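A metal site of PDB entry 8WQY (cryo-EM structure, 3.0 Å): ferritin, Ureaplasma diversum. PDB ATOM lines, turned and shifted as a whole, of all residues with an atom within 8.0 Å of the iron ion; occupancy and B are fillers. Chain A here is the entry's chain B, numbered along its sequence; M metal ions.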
ATOM      1  N   ASN A  27       6.268  -6.780  16.310  1.00  0.00           N
ATOM      2  CA  ASN A  27       6.536  -5.681  17.222  1.00  0.00           C
ATOM      3  C   ASN A  27       5.876  -4.390  16.753  1.00  0.00           C
ATOM      4  O   ASN A  27       5.274  -3.661  17.565  1.00  0.00           O
ATOM      5  CB  ASN A  27       8.044  -5.489  17.386  1.00  0.00           C
ATOM      6  CG  ASN A  27       8.648  -6.447  18.385  1.00  0.00           C
ATOM      7  OD1 ASN A  27       9.003  -6.050  19.497  1.00  0.00           O
ATOM      8  ND2 ASN A  27       8.747  -7.709  18.019  1.00  0.00           N
ATOM      9  N   HIS A  56       3.873   3.850  27.831  1.00  0.00           N
ATOM     10  CA  HIS A  56       5.228   3.365  28.058  1.00  0.00           C
ATOM     11  C   HIS A  56       5.458   2.053  27.316  1.00  0.00           C
ATOM     12  O   HIS A  56       6.471   1.884  26.624  1.00  0.00           O
ATOM     13  CB  HIS A  56       5.499   3.196  29.549  1.00  0.00           C
ATOM     14  CG  HIS A  56       5.784   4.467  30.272  1.00  0.00           C
ATOM     15  ND1 HIS A  56       4.796   5.343  30.659  1.00  0.00           N
ATOM     16  CD2 HIS A  56       6.951   5.003  30.704  1.00  0.00           C
ATOM     17  CE1 HIS A  56       5.338   6.374  31.282  1.00  0.00           C
ATOM     18  NE2 HIS A  56       6.645   6.198  31.328  1.00  0.00           N
ATOM     19  N   LEU A  57       4.515   1.125  27.455  1.00  0.00           N
ATOM     20  CA  LEU A  57       4.655  -0.157  26.747  1.00  0.00           C
ATOM     21  C   LEU A  57       4.758   0.034  25.238  1.00  0.00           C
ATOM     22  O   LEU A  57       5.595  -0.582  24.585  1.00  0.00           O
ATOM     23  CB  LEU A  57       3.484  -1.080  27.080  1.00  0.00           C
ATOM     24  CG  LEU A  57       3.624  -1.952  28.328  1.00  0.00           C
ATOM     25  CD1 LEU A  57       2.400  -2.815  28.501  1.00  0.00           C
ATOM     26  CD2 LEU A  57       4.865  -2.810  28.219  1.00  0.00           C
ATOM     27  N   GLU A  59       5.660   2.729  23.406  1.00  0.00           N
ATOM     28  CA  GLU A  59       6.926   3.326  23.002  1.00  0.00           C
ATOM     29  C   GLU A  59       8.056   2.323  23.108  1.00  0.00           C
ATOM     30  O   GLU A  59       8.953   2.289  22.248  1.00  0.00           O
ATOM     31  CB  GLU A  59       7.221   4.560  23.851  1.00  0.00           C
ATOM     32  CG  GLU A  59       6.518   5.820  23.379  1.00  0.00           C
ATOM     33  CD  GLU A  59       6.682   6.956  24.366  1.00  0.00           C
ATOM     34  OE1 GLU A  59       6.057   8.026  24.159  1.00  0.00           O
ATOM     35  OE2 GLU A  59       7.427   6.780  25.350  1.00  0.00           O
ATOM     36  N   ASP A  60       8.046   1.500  24.153  1.00  0.00           N
ATOM     37  CA  ASP A  60       9.097   0.500  24.309  1.00  0.00           C
ATOM     38  C   ASP A  60       9.048  -0.533  23.193  1.00  0.00           C
ATOM     39  O   ASP A  60      10.092  -1.023  22.755  1.00  0.00           O
ATOM     40  CB  ASP A  60       8.964  -0.179  25.670  1.00  0.00           C
ATOM     41  CG  ASP A  60       9.849  -1.390  25.809  1.00  0.00           C
ATOM     42  OD1 ASP A  60      11.010  -1.346  25.353  1.00  0.00           O
ATOM     43  OD2 ASP A  60       9.389  -2.403  26.384  1.00  0.00           O
ATOM     44  N   LYS A  61       7.858  -0.857  22.695  1.00  0.00           N
ATOM     45  CA  LYS A  61       7.782  -1.795  21.569  1.00  0.00           C
ATOM     46  C   LYS A  61       8.256  -1.144  20.272  1.00  0.00           C
ATOM     47  O   LYS A  61       9.009  -1.752  19.517  1.00  0.00           O
ATOM     48  CB  LYS A  61       6.361  -2.318  21.400  1.00  0.00           C
ATOM     49  CG  LYS A  61       5.849  -3.092  22.597  1.00  0.00           C
ATOM     50  CD  LYS A  61       6.715  -4.300  22.874  1.00  0.00           C
ATOM     51  CE  LYS A  61       6.304  -4.939  24.183  1.00  0.00           C
ATOM     52  NZ  LYS A  61       6.720  -6.364  24.246  1.00  0.00           N
ATOM     53  N   VAL A  64      13.412   0.427  20.931  1.00  0.00           N
ATOM     54  CA  VAL A  64      14.593  -0.432  20.947  1.00  0.00           C
ATOM     55  C   VAL A  64      14.258  -1.848  20.501  1.00  0.00           C
ATOM     56  O   VAL A  64      15.075  -2.506  19.850  1.00  0.00           O
ATOM     57  CB  VAL A  64      15.254  -0.409  22.336  1.00  0.00           C
ATOM     58  CG1 VAL A  64      15.518   1.007  22.770  1.00  0.00           C
ATOM     59  CG2 VAL A  64      14.369  -1.098  23.359  1.00  0.00           C
ATOM     60  N   HIS A  65      13.051  -2.322  20.819  1.00  0.00           N
ATOM     61  CA  HIS A  65      12.688  -3.706  20.529  1.00  0.00           C
ATOM     62  C   HIS A  65      12.826  -4.052  19.057  1.00  0.00           C
ATOM     63  O   HIS A  65      12.986  -5.225  18.709  1.00  0.00           O
ATOM     64  CB  HIS A  65      11.272  -3.993  21.012  1.00  0.00           C
ATOM     65  CG  HIS A  65      11.196  -4.586  22.383  1.00  0.00           C
ATOM     66  ND1 HIS A  65      11.206  -5.944  22.602  1.00  0.00           N
ATOM     67  CD2 HIS A  65      11.106  -4.018  23.608  1.00  0.00           C
ATOM     68  CE1 HIS A  65      11.123  -6.189  23.897  1.00  0.00           C
ATOM     69  NE2 HIS A  65      11.065  -5.039  24.530  1.00  0.00           N
ATOM     70  N   GLU A 106       1.350 -10.306  25.534  1.00  0.00           N
ATOM     71  CA  GLU A 106       2.691 -10.557  26.048  1.00  0.00           C
ATOM     72  C   GLU A 106       2.977 -12.053  26.156  1.00  0.00           C
ATOM     73  O   GLU A 106       4.081 -12.518  25.820  1.00  0.00           O
ATOM     74  CB  GLU A 106       2.870  -9.879  27.405  1.00  0.00           C
ATOM     75  CG  GLU A 106       2.761  -8.367  27.368  1.00  0.00           C
ATOM     76  CD  GLU A 106       3.731  -7.721  26.412  1.00  0.00           C
ATOM     77  OE1 GLU A 106       4.812  -8.301  26.165  1.00  0.00           O
ATOM     78  OE2 GLU A 106       3.421  -6.636  25.890  1.00  0.00           O
ATOM     79  N   TRP A 134      18.803 -11.622  24.985  1.00  0.00           N
ATOM     80  CA  TRP A 134      18.230 -10.359  25.435  1.00  0.00           C
ATOM     81  C   TRP A 134      16.717 -10.380  25.376  1.00  0.00           C
ATOM     82  O   TRP A 134      16.038  -9.929  26.316  1.00  0.00           O
ATOM     83  CB  TRP A 134      18.785  -9.213  24.587  1.00  0.00           C
ATOM     84  CG  TRP A 134      18.534  -7.853  25.146  1.00  0.00           C
ATOM     85  CD1 TRP A 134      19.402  -7.109  25.888  1.00  0.00           C
ATOM     86  CD2 TRP A 134      17.356  -7.062  24.989  1.00  0.00           C
ATOM     87  NE1 TRP A 134      18.832  -5.906  26.217  1.00  0.00           N
ATOM     88  CE2 TRP A 134      17.568  -5.853  25.678  1.00  0.00           C
ATOM     89  CE3 TRP A 134      16.134  -7.250  24.340  1.00  0.00           C
ATOM     90  CZ2 TRP A 134      16.615  -4.843  25.728  1.00  0.00           C
ATOM     91  CZ3 TRP A 134      15.194  -6.257  24.402  1.00  0.00           C
ATOM     92  CH2 TRP A 134      15.436  -5.061  25.092  1.00  0.00           C
ATOM     93  N   TYR A 135      16.154 -10.887  24.278  1.00  0.00           N
ATOM     94  CA  TYR A 135      14.705 -10.938  24.152  1.00  0.00           C
ATOM     95  C   TYR A 135      14.120 -11.959  25.122  1.00  0.00           C
ATOM     96  O   TYR A 135      13.048 -11.727  25.691  1.00  0.00           O
ATOM     97  CB  TYR A 135      14.318 -11.278  22.717  1.00  0.00           C
ATOM     98  CG  TYR A 135      14.519 -10.146  21.746  1.00  0.00           C
ATOM     99  CD1 TYR A 135      15.788  -9.749  21.355  1.00  0.00           C
ATOM    100  CD2 TYR A 135      13.436  -9.457  21.237  1.00  0.00           C
ATOM    101  CE1 TYR A 135      15.961  -8.717  20.480  1.00  0.00           C
ATOM    102  CE2 TYR A 135      13.611  -8.416  20.359  1.00  0.00           C
ATOM    103  CZ  TYR A 135      14.877  -8.056  19.982  1.00  0.00           C
ATOM    104  OH  TYR A 135      15.047  -7.018  19.096  1.00  0.00           O
ATOM    105  N   ARG A 137      15.156 -12.556  28.078  1.00  0.00           N
ATOM    106  CA  ARG A 137      15.063 -11.904  29.381  1.00  0.00           C
ATOM    107  C   ARG A 137      13.966 -10.842  29.402  1.00  0.00           C
ATOM    108  O   ARG A 137      13.124 -10.820  30.321  1.00  0.00           O
ATOM    109  CB  ARG A 137      16.413 -11.275  29.723  1.00  0.00           C
ATOM    110  CG  ARG A 137      16.407 -10.443  30.975  1.00  0.00           C
ATOM    111  CD  ARG A 137      17.745  -9.761  31.151  1.00  0.00           C
ATOM    112  NE  ARG A 137      18.040  -8.849  30.048  1.00  0.00           N
ATOM    113  CZ  ARG A 137      17.672  -7.572  30.026  1.00  0.00           C
ATOM    114  NH1 ARG A 137      16.998  -7.049  31.043  1.00  0.00           N
ATOM    115  NH2 ARG A 137      17.980  -6.810  28.983  1.00  0.00           N
ATOM    116  N   ASP A 138      13.959  -9.952  28.411  1.00  0.00           N
ATOM    117  CA  ASP A 138      13.033  -8.834  28.467  1.00  0.00           C
ATOM    118  C   ASP A 138      11.587  -9.280  28.353  1.00  0.00           C
ATOM    119  O   ASP A 138      10.692  -8.599  28.859  1.00  0.00           O
ATOM    120  CB  ASP A 138      13.359  -7.820  27.382  1.00  0.00           C
ATOM    121  CG  ASP A 138      12.758  -6.454  27.656  1.00  0.00           C
ATOM    122  OD1 ASP A 138      13.281  -5.756  28.551  1.00  0.00           O
ATOM    123  OD2 ASP A 138      11.771  -6.081  26.991  1.00  0.00           O
ATOM    124  N   GLY A 139      11.331 -10.433  27.714  1.00  0.00           N
ATOM    125  CA  GLY A 139       9.965 -10.935  27.662  1.00  0.00           C
ATOM    126  C   GLY A 139       9.401 -11.211  29.044  1.00  0.00           C
ATOM    127  O   GLY A 139       8.292 -10.768  29.379  1.00  0.00           O
ATOM    128  N   LYS A 141      10.565 -10.024  31.875  1.00  0.00           N
ATOM    129  CA  LYS A 141      10.490  -8.764  32.618  1.00  0.00           C
ATOM    130  C   LYS A 141       9.191  -8.026  32.306  1.00  0.00           C
ATOM    131  O   LYS A 141       8.483  -7.553  33.217  1.00  0.00           O
ATOM    132  CB  LYS A 141      11.703  -7.891  32.305  1.00  0.00           C
ATOM    133  CG  LYS A 141      11.650  -6.526  32.964  1.00  0.00           C
ATOM    134  CD  LYS A 141      12.421  -5.500  32.145  1.00  0.00           C
ATOM    135  CE  LYS A 141      11.974  -4.083  32.465  1.00  0.00           C
ATOM    136  NZ  LYS A 141      12.297  -3.141  31.360  1.00  0.00           N
ATOM    137  N   ASP A 142       8.841  -7.908  31.026  1.00  0.00           N
ATOM    138  CA  ASP A 142       7.618  -7.209  30.655  1.00  0.00           C
ATOM    139  C   ASP A 142       6.386  -7.950  31.164  1.00  0.00           C
ATOM    140  O   ASP A 142       5.431  -7.314  31.657  1.00  0.00           O
ATOM    141  CB  ASP A 142       7.537  -7.040  29.140  1.00  0.00           C
ATOM    142  CG  ASP A 142       8.424  -5.931  28.633  1.00  0.00           C
ATOM    143  OD1 ASP A 142       9.165  -5.343  29.448  1.00  0.00           O
ATOM    144  OD2 ASP A 142       8.384  -5.645  27.420  1.00  0.00           O
ATOM    145  N   GLU A 145       6.009  -7.232  34.890  1.00  0.00           N
ATOM    146  CA  GLU A 145       5.620  -5.877  35.226  1.00  0.00           C
ATOM    147  C   GLU A 145       4.210  -5.545  34.740  1.00  0.00           C
ATOM    148  O   GLU A 145       3.652  -4.536  35.181  1.00  0.00           O
ATOM    149  CB  GLU A 145       6.604  -4.863  34.658  1.00  0.00           C
ATOM    150  CG  GLU A 145       6.484  -4.625  33.174  1.00  0.00           C
ATOM    151  CD  GLU A 145       7.223  -3.371  32.735  1.00  0.00           C
ATOM    152  OE1 GLU A 145       7.211  -3.064  31.524  1.00  0.00           O
ATOM    153  OE2 GLU A 145       7.817  -2.699  33.604  1.00  0.00           O
HETATM  154 FE    FE M   1      10.796  -4.354  26.403  1.00  0.00          FE
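OD2 of Asp 142 lies within salt-bridge range of NZ of Lys 61 (3.7 Å). OD1 of Asp 138 is in salt-bridge range of NZ of Lys 141 (3.96 Å). The backbone carbonyl oxygen of His 65 sits at hydrogen-bond distance from the side-chain hydroxyl of Tyr 135 (2.8 Å).
Asp 142 touches the iron ion. Within 4 Å of the iron ion: Asp 60, His 65, Asp 138 and Asp 142. The nearest printed residue that does not touch the iron ion is Trp 134 (4.9 Å).
A ring nitrogen (NE2) of His 65 is bound to the iron ion, at 2.0 Å. The iron ion is bound by the side-chain carboxylate (OD2) of Asp 138 (2.1 Å). The side-chain carboxylate (OD2) of Asp 60 is bound to the iron ion (2.4 Å).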
